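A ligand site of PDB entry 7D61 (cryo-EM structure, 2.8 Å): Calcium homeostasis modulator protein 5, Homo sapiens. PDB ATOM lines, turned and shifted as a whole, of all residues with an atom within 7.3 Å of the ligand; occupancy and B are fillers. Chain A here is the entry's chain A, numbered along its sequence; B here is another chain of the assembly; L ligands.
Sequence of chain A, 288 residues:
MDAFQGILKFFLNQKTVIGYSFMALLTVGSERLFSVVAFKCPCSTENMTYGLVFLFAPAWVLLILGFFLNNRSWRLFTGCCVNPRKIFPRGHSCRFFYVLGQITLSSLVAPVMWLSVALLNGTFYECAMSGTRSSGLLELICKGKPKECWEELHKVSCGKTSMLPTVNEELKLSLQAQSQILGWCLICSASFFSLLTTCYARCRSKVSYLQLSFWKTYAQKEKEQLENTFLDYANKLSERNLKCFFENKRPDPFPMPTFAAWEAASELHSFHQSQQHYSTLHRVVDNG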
ATOM      1  N   ALA A  24      27.320  30.249   4.182  1.00  0.00           N
ATOM      2  CA  ALA A  24      26.757  29.657   2.974  1.00  0.00           C
ATOM      3  C   ALA A  24      25.246  29.503   3.053  1.00  0.00           C
ATOM      4  O   ALA A  24      24.570  29.519   2.012  1.00  0.00           O
ATOM      5  CB  ALA A  24      27.399  28.291   2.713  1.00  0.00           C
ATOM      6  N   LEU A  25      24.689  29.368   4.254  1.00  0.00           N
ATOM      7  CA  LEU A  25      23.251  29.252   4.403  1.00  0.00           C
ATOM      8  C   LEU A  25      22.544  30.597   4.278  1.00  0.00           C
ATOM      9  O   LEU A  25      21.344  30.634   3.992  1.00  0.00           O
ATOM     10  CB  LEU A  25      22.934  28.600   5.757  1.00  0.00           C
ATOM     11  CG  LEU A  25      21.535  28.095   6.135  1.00  0.00           C
ATOM     12  CD1 LEU A  25      21.653  26.852   6.982  1.00  0.00           C
ATOM     13  CD2 LEU A  25      20.741  29.145   6.902  1.00  0.00           C
ATOM     14  N   VAL A  28      22.344  31.543   0.243  1.00  0.00           N
ATOM     15  CA  VAL A  28      21.290  30.815  -0.462  1.00  0.00           C
ATOM     16  C   VAL A  28      19.935  31.486  -0.245  1.00  0.00           C
ATOM     17  O   VAL A  28      19.169  31.681  -1.188  1.00  0.00           O
ATOM     18  CB  VAL A  28      21.288  29.338  -0.016  1.00  0.00           C
ATOM     19  CG1 VAL A  28      20.061  28.613  -0.538  1.00  0.00           C
ATOM     20  CG2 VAL A  28      22.558  28.652  -0.499  1.00  0.00           C
ATOM     21  N   GLY A  29      19.644  31.870   0.999  1.00  0.00           N
ATOM     22  CA  GLY A  29      18.392  32.545   1.280  1.00  0.00           C
ATOM     23  C   GLY A  29      18.339  33.975   0.788  1.00  0.00           C
ATOM     24  O   GLY A  29      17.234  34.520   0.633  1.00  0.00           O
ATOM     25  N   GLU A  31      19.780  34.824  -2.183  1.00  0.00           N
ATOM     26  CA  GLU A  31      19.671  34.717  -3.634  1.00  0.00           C
ATOM     27  C   GLU A  31      18.308  34.204  -4.077  1.00  0.00           C
ATOM     28  O   GLU A  31      17.887  34.501  -5.200  1.00  0.00           O
ATOM     29  CB  GLU A  31      20.759  33.786  -4.167  1.00  0.00           C
ATOM     30  CG  GLU A  31      21.150  34.051  -5.611  1.00  0.00           C
ATOM     31  CD  GLU A  31      20.369  33.204  -6.596  1.00  0.00           C
ATOM     32  OE1 GLU A  31      19.747  32.221  -6.163  1.00  0.00           O
ATOM     33  OE2 GLU A  31      20.377  33.539  -7.795  1.00  0.00           O
ATOM     34  N   ARG A  32      17.597  33.486  -3.216  1.00  0.00           N
ATOM     35  CA  ARG A  32      16.231  33.052  -3.505  1.00  0.00           C
ATOM     36  C   ARG A  32      15.194  34.109  -3.142  1.00  0.00           C
ATOM     37  O   ARG A  32      14.002  33.820  -3.168  1.00  0.00           O
ATOM     38  CB  ARG A  32      15.914  31.745  -2.768  1.00  0.00           C
ATOM     39  CG  ARG A  32      16.712  30.562  -3.281  1.00  0.00           C
ATOM     40  CD  ARG A  32      16.548  30.407  -4.777  1.00  0.00           C
ATOM     41  NE  ARG A  32      15.174  30.081  -5.149  1.00  0.00           N
ATOM     42  CZ  ARG A  32      14.538  30.596  -6.202  1.00  0.00           C
ATOM     43  NH1 ARG A  32      15.152  31.473  -6.983  1.00  0.00           N
ATOM     44  NH2 ARG A  32      13.291  30.244  -6.464  1.00  0.00           N
ATOM     45  N   SER A  35      15.908  36.923  -6.872  1.00  0.00           N
ATOM     46  CA  SER A  35      15.413  36.400  -8.138  1.00  0.00           C
ATOM     47  C   SER A  35      13.916  36.132  -8.135  1.00  0.00           C
ATOM     48  O   SER A  35      13.328  35.984  -9.214  1.00  0.00           O
ATOM     49  CB  SER A  35      16.165  35.114  -8.498  1.00  0.00           C
ATOM     50  OG  SER A  35      15.606  34.000  -7.814  1.00  0.00           O
ATOM     51  N   VAL A  36      13.294  36.069  -6.967  1.00  0.00           N
ATOM     52  CA  VAL A  36      11.866  35.774  -6.852  1.00  0.00           C
ATOM     53  C   VAL A  36      11.033  37.046  -6.749  1.00  0.00           C
ATOM     54  O   VAL A  36      10.011  37.179  -7.417  1.00  0.00           O
ATOM     55  CB  VAL A  36      11.638  34.834  -5.639  1.00  0.00           C
ATOM     56  CG1 VAL A  36      10.170  34.803  -5.224  1.00  0.00           C
ATOM     57  CG2 VAL A  36      12.143  33.434  -5.954  1.00  0.00           C
ATOM     58  N   SER A 116      28.415  31.372  -7.183  1.00  0.00           N
ATOM     59  CA  SER A 116      28.114  29.973  -7.405  1.00  0.00           C
ATOM     60  C   SER A 116      26.632  29.671  -7.208  1.00  0.00           C
ATOM     61  O   SER A 116      26.056  28.898  -7.982  1.00  0.00           O
ATOM     62  CB  SER A 116      28.951  29.098  -6.479  1.00  0.00           C
ATOM     63  OG  SER A 116      30.327  29.347  -6.653  1.00  0.00           O
ATOM     64  N   VAL A 117      26.010  30.254  -6.187  1.00  0.00           N
ATOM     65  CA  VAL A 117      24.579  30.052  -5.967  1.00  0.00           C
ATOM     66  C   VAL A 117      23.769  30.810  -7.025  1.00  0.00           C
ATOM     67  O   VAL A 117      22.703  30.342  -7.447  1.00  0.00           O
ATOM     68  CB  VAL A 117      24.223  30.478  -4.527  1.00  0.00           C
ATOM     69  CG1 VAL A 117      22.747  30.271  -4.230  1.00  0.00           C
ATOM     70  CG2 VAL A 117      25.054  29.689  -3.541  1.00  0.00           C
ATOM     71  N   LEU A 119      24.724  31.290 -10.131  1.00  0.00           N
ATOM     72  CA  LEU A 119      24.856  30.570 -11.389  1.00  0.00           C
ATOM     73  C   LEU A 119      24.201  29.195 -11.359  1.00  0.00           C
ATOM     74  O   LEU A 119      23.869  28.656 -12.420  1.00  0.00           O
ATOM     75  CB  LEU A 119      26.333  30.416 -11.766  1.00  0.00           C
ATOM     76  CG  LEU A 119      26.977  31.590 -12.484  1.00  0.00           C
ATOM     77  CD1 LEU A 119      28.460  31.341 -12.682  1.00  0.00           C
ATOM     78  CD2 LEU A 119      26.291  31.842 -13.803  1.00  0.00           C
ATOM     79  N   LEU A 120      23.983  28.617 -10.180  1.00  0.00           N
ATOM     80  CA  LEU A 120      23.234  27.369 -10.059  1.00  0.00           C
ATOM     81  C   LEU A 120      21.729  27.591 -10.072  1.00  0.00           C
ATOM     82  O   LEU A 120      20.972  26.613 -10.029  1.00  0.00           O
ATOM     83  CB  LEU A 120      23.641  26.628  -8.789  1.00  0.00           C
ATOM     84  CG  LEU A 120      24.971  25.866  -8.818  1.00  0.00           C
ATOM     85  CD1 LEU A 120      25.202  25.159  -7.507  1.00  0.00           C
ATOM     86  CD2 LEU A 120      25.000  24.893  -9.976  1.00  0.00           C
ATOM     87  N   ASN A 121      21.282  28.835 -10.098  1.00  0.00           N
ATOM     88  CA  ASN A 121      19.888  29.217 -10.309  1.00  0.00           C
ATOM     89  C   ASN A 121      19.923  30.111 -11.538  1.00  0.00           C
ATOM     90  O   ASN A 121      20.097  31.331 -11.428  1.00  0.00           O
ATOM     91  CB  ASN A 121      19.303  29.901  -9.066  1.00  0.00           C
ATOM     92  CG  ASN A 121      17.974  30.565  -9.331  1.00  0.00           C
ATOM     93  OD1 ASN A 121      17.144  30.059 -10.095  1.00  0.00           O
ATOM     94  ND2 ASN A 121      17.743  31.715  -8.694  1.00  0.00           N
ATOM     95  N   GLY A 122      19.773  29.514 -12.714  1.00  0.00           N
ATOM     96  CA  GLY A 122      20.113  30.182 -13.953  1.00  0.00           C
ATOM     97  C   GLY A 122      19.121  31.207 -14.463  1.00  0.00           C
ATOM     98  O   GLY A 122      18.656  31.099 -15.600  1.00  0.00           O
ATOM     99  N   THR A 123      18.789  32.200 -13.647  1.00  0.00           N
ATOM    100  CA  THR A 123      17.901  33.280 -14.072  1.00  0.00           C
ATOM    101  C   THR A 123      18.653  34.550 -14.459  1.00  0.00           C
ATOM    102  O   THR A 123      18.169  35.312 -15.298  1.00  0.00           O
ATOM    103  CB  THR A 123      16.895  33.608 -12.970  1.00  0.00           C
ATOM    104  OG1 THR A 123      17.567  34.272 -11.884  1.00  0.00           O
ATOM    105  CG2 THR A 123      16.238  32.346 -12.455  1.00  0.00           C
ATOM    106  N   GLN A 176      19.458  27.724 -19.419  1.00  0.00           N
ATOM    107  CA  GLN A 176      19.412  27.405 -17.993  1.00  0.00           C
ATOM    108  C   GLN A 176      20.288  26.207 -17.650  1.00  0.00           C
ATOM    109  O   GLN A 176      20.342  25.816 -16.488  1.00  0.00           O
ATOM    110  CB  GLN A 176      17.964  27.142 -17.580  1.00  0.00           C
ATOM    111  CG  GLN A 176      17.605  27.570 -16.163  1.00  0.00           C
ATOM    112  CD  GLN A 176      17.493  26.388 -15.217  1.00  0.00           C
ATOM    113  OE1 GLN A 176      17.215  25.265 -15.633  1.00  0.00           O
ATOM    114  NE2 GLN A 176      17.713  26.652 -13.928  1.00  0.00           N
ATOM    115  N   GLN A 180      24.497  26.323 -15.146  1.00  0.00           N
ATOM    116  CA  GLN A 180      24.718  25.349 -14.080  1.00  0.00           C
ATOM    117  C   GLN A 180      25.963  24.506 -14.324  1.00  0.00           C
ATOM    118  O   GLN A 180      26.524  23.964 -13.377  1.00  0.00           O
ATOM    119  CB  GLN A 180      23.483  24.455 -13.933  1.00  0.00           C
ATOM    120  CG  GLN A 180      22.267  25.213 -13.453  1.00  0.00           C
ATOM    121  CD  GLN A 180      21.064  24.313 -13.279  1.00  0.00           C
ATOM    122  OE1 GLN A 180      20.817  23.421 -14.082  1.00  0.00           O
ATOM    123  NE2 GLN A 180      20.291  24.547 -12.229  1.00  0.00           N
ATOM    124  N   TRP A 184      29.184  24.788 -11.439  1.00  0.00           N
ATOM    125  CA  TRP A 184      29.986  23.729 -10.840  1.00  0.00           C
ATOM    126  C   TRP A 184      31.464  23.850 -11.206  1.00  0.00           C
ATOM    127  O   TRP A 184      32.303  23.309 -10.486  1.00  0.00           O
ATOM    128  CB  TRP A 184      29.479  22.357 -11.252  1.00  0.00           C
ATOM    129  CG  TRP A 184      28.189  21.943 -10.602  1.00  0.00           C
ATOM    130  CD1 TRP A 184      26.998  21.712 -11.216  1.00  0.00           C
ATOM    131  CD2 TRP A 184      27.969  21.694  -9.209  1.00  0.00           C
ATOM    132  NE1 TRP A 184      26.051  21.352 -10.301  1.00  0.00           N
ATOM    133  CE2 TRP A 184      26.616  21.339  -9.057  1.00  0.00           C
ATOM    134  CE3 TRP A 184      28.778  21.757  -8.066  1.00  0.00           C
ATOM    135  CZ2 TRP A 184      26.064  21.039  -7.817  1.00  0.00           C
ATOM    136  CZ3 TRP A 184      28.229  21.458  -6.840  1.00  0.00           C
ATOM    137  CH2 TRP A 184      26.876  21.106  -6.724  1.00  0.00           C
ATOM    138  N   LEU B  33      17.233  16.930  -3.033  1.00  0.00           N
ATOM    139  CA  LEU B  33      16.993  18.351  -3.237  1.00  0.00           C
ATOM    140  C   LEU B  33      17.644  18.877  -4.503  1.00  0.00           C
ATOM    141  O   LEU B  33      17.155  19.861  -5.063  1.00  0.00           O
ATOM    142  CB  LEU B  33      17.473  19.152  -2.021  1.00  0.00           C
ATOM    143  CG  LEU B  33      17.154  20.637  -1.818  1.00  0.00           C
ATOM    144  CD1 LEU B  33      16.965  20.898  -0.336  1.00  0.00           C
ATOM    145  CD2 LEU B  33      18.270  21.529  -2.352  1.00  0.00           C
ATOM    146  N   PHE B  34      18.736  18.258  -4.969  1.00  0.00           N
ATOM    147  CA  PHE B  34      19.348  18.663  -6.229  1.00  0.00           C
ATOM    148  C   PHE B  34      18.528  18.173  -7.417  1.00  0.00           C
ATOM    149  O   PHE B  34      18.402  18.895  -8.416  1.00  0.00           O
ATOM    150  CB  PHE B  34      20.775  18.138  -6.319  1.00  0.00           C
ATOM    151  CG  PHE B  34      21.804  19.068  -5.762  1.00  0.00           C
ATOM    152  CD1 PHE B  34      21.878  20.375  -6.199  1.00  0.00           C
ATOM    153  CD2 PHE B  34      22.695  18.629  -4.794  1.00  0.00           C
ATOM    154  CE1 PHE B  34      22.832  21.242  -5.686  1.00  0.00           C
ATOM    155  CE2 PHE B  34      23.657  19.487  -4.273  1.00  0.00           C
ATOM    156  CZ  PHE B  34      23.712  20.791  -4.722  1.00  0.00           C
ATOM    157  N   VAL B  36      15.201  17.283  -7.383  1.00  0.00           N
ATOM    158  CA  VAL B  36      13.821  17.717  -7.331  1.00  0.00           C
ATOM    159  C   VAL B  36      13.686  19.192  -7.688  1.00  0.00           C
ATOM    160  O   VAL B  36      12.805  19.575  -8.457  1.00  0.00           O
ATOM    161  CB  VAL B  36      13.240  17.419  -5.929  1.00  0.00           C
ATOM    162  CG1 VAL B  36      11.971  18.223  -5.643  1.00  0.00           C
ATOM    163  CG2 VAL B  36      12.960  15.932  -5.779  1.00  0.00           C
ATOM    164  N   VAL B  37      14.598  20.032  -7.194  1.00  0.00           N
ATOM    165  CA  VAL B  37      14.444  21.481  -7.276  1.00  0.00           C
ATOM    166  C   VAL B  37      15.338  22.088  -8.345  1.00  0.00           C
ATOM    167  O   VAL B  37      14.912  22.994  -9.062  1.00  0.00           O
ATOM    168  CB  VAL B  37      14.725  22.094  -5.875  1.00  0.00           C
ATOM    169  CG1 VAL B  37      14.453  23.575  -5.882  1.00  0.00           C
ATOM    170  CG2 VAL B  37      13.893  21.398  -4.818  1.00  0.00           C
ATOM    171  N   ALA B  38      16.560  21.590  -8.495  1.00  0.00           N
ATOM    172  CA  ALA B  38      17.543  22.229  -9.362  1.00  0.00           C
ATOM    173  C   ALA B  38      17.754  21.531 -10.696  1.00  0.00           C
ATOM    174  O   ALA B  38      18.067  22.203 -11.678  1.00  0.00           O
ATOM    175  CB  ALA B  38      18.893  22.339  -8.643  1.00  0.00           C
ATOM    176  N   PHE B  39      17.602  20.209 -10.755  1.00  0.00           N
ATOM    177  CA  PHE B  39      17.898  19.456 -11.963  1.00  0.00           C
ATOM    178  C   PHE B  39      16.680  19.470 -12.880  1.00  0.00           C
ATOM    179  O   PHE B  39      15.570  19.120 -12.469  1.00  0.00           O
ATOM    180  CB  PHE B  39      18.298  18.023 -11.613  1.00  0.00           C
ATOM    181  CG  PHE B  39      18.874  17.248 -12.775  1.00  0.00           C
ATOM    182  CD1 PHE B  39      18.064  16.452 -13.563  1.00  0.00           C
ATOM    183  CD2 PHE B  39      20.234  17.298 -13.049  1.00  0.00           C
ATOM    184  CE1 PHE B  39      18.585  15.729 -14.620  1.00  0.00           C
ATOM    185  CE2 PHE B  39      20.761  16.576 -14.098  1.00  0.00           C
ATOM    186  CZ  PHE B  39      19.941  15.799 -14.893  1.00  0.00           C
ATOM    187  N   LYS B  40      16.892  19.879 -14.132  1.00  0.00           N
ATOM    188  CA  LYS B  40      15.894  19.732 -15.184  1.00  0.00           C
ATOM    189  C   LYS B  40      16.628  19.501 -16.495  1.00  0.00           C
ATOM    190  O   LYS B  40      17.359  20.375 -16.970  1.00  0.00           O
ATOM    191  CB  LYS B  40      14.942  20.933 -15.251  1.00  0.00           C
ATOM    192  CG  LYS B  40      15.580  22.311 -15.103  1.00  0.00           C
ATOM    193  CD  LYS B  40      14.514  23.386 -15.019  1.00  0.00           C
ATOM    194  CE  LYS B  40      13.796  23.351 -13.671  1.00  0.00           C
ATOM    195  NZ  LYS B  40      14.693  23.739 -12.552  1.00  0.00           N
HETATM  196  O1  LIG L   1      14.033  26.093  -9.663  1.00  0.00           O
HETATM  197  O2  LIG L   1      16.489  26.279  -9.890  1.00  0.00           O
HETATM  198  P1  LIG L   1      15.217  27.043  -9.624  1.00  0.00           P
HETATM  199  O3  LIG L   1      15.040  28.098 -10.687  1.00  0.00           O
HETATM  200  O4  LIG L   1      15.294  27.754  -8.143  1.00  0.00           O
HETATM  201  C1  LIG L   1      16.522  27.783  -7.473  1.00  0.00           C
HETATM  202  C2  LIG L   1      16.547  26.633  -6.474  1.00  0.00           C
HETATM  203  C3  LIG L   1      17.906  25.931  -6.549  1.00  0.00           C
HETATM  204  O5  LIG L   1      18.483  25.938  -5.278  1.00  0.00           O
HETATM  205  C4  LIG L   1      19.870  25.714  -5.260  1.00  0.00           C
HETATM  206  O6  LIG L   1      20.478  25.629  -6.281  1.00  0.00           O
HETATM  207  C5  LIG L   1      20.608  25.573  -3.931  1.00  0.00           C
HETATM  208  C6  LIG L   1      22.096  25.295  -4.132  1.00  0.00           C
HETATM  209  C7  LIG L   1      22.764  24.758  -2.873  1.00  0.00           C
HETATM  210  O7  LIG L   1      16.336  27.109  -5.166  1.00  0.00           O
HETATM  211  C8  LIG L   1      15.037  26.929  -4.663  1.00  0.00           C
HETATM  212  O8  LIG L   1      14.111  26.851  -5.395  1.00  0.00           O
HETATM  213  C9  LIG L   1      14.807  26.842  -3.152  1.00  0.00           C
HETATM  214  C10 LIG L   1      15.449  25.626  -2.502  1.00  0.00           C
HETATM  215  C11 LIG L   1      16.919  25.850  -2.152  1.00  0.00           C
HETATM  216  C12 LIG L   1      17.407  24.952  -1.023  1.00  0.00           C
HETATM  217  C13 LIG L   1      16.845  25.356   0.337  1.00  0.00           C
HETATM  218  C14 LIG L   1      17.586  24.669   1.484  1.00  0.00           C
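An oxygen (O3) of the ligand sits close to the side-chain amide oxygen (OD1) of Asn 121, at 2.9 Å.
The guanidinium group (NE) of Arg 32 sits at hydrogen-bond distance from an oxygen (O7) of the ligand, at 3.2 Å.
O1 of the ligand lies within salt-bridge range of NZ of Lys 40 of chain B, at 3.8 Å.
The guanidinium group of Arg 32 lies close to the side-chain amide nitrogen of Asn 121 (3.1 Å).
The side-chain amide nitrogen (ND2) of Asn 121 lies within hydrogen-bond range of the side-chain carboxylate (OE1) of Glu 31.
The side-chain amide nitrogen (ND2) of Asn 121 sits at hydrogen-bond distance from the side-chain hydroxyl (OG) of Ser 35 (3.2 Å).
OG of Ser 35 is in hydrogen-bond range of NH1 of Arg 32, 2.7 Å away.
The side-chain amide nitrogen (NE2) of Gln 180 lies within hydrogen-bond range of the backbone carbonyl oxygen (O) of Leu 120 (3.1 Å).
The backbone carbonyl oxygen (O) of Val 37 of chain B sits close to an oxygen (O1) of the ligand (3.3 Å).
O of Leu 120 touches O6 of the ligand, at 3.9 Å.
CD2 of Leu 33 of chain B touches C12 of the ligand, 3.8 Å away.
Hydrophobic or aromatic side chains within 4 Å of the ligand: Leu 33 of chain B and Val 37 of chain B.
The nearest printed residue that does not touch the ligand is Ala 38 of chain B (4.2 Å).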
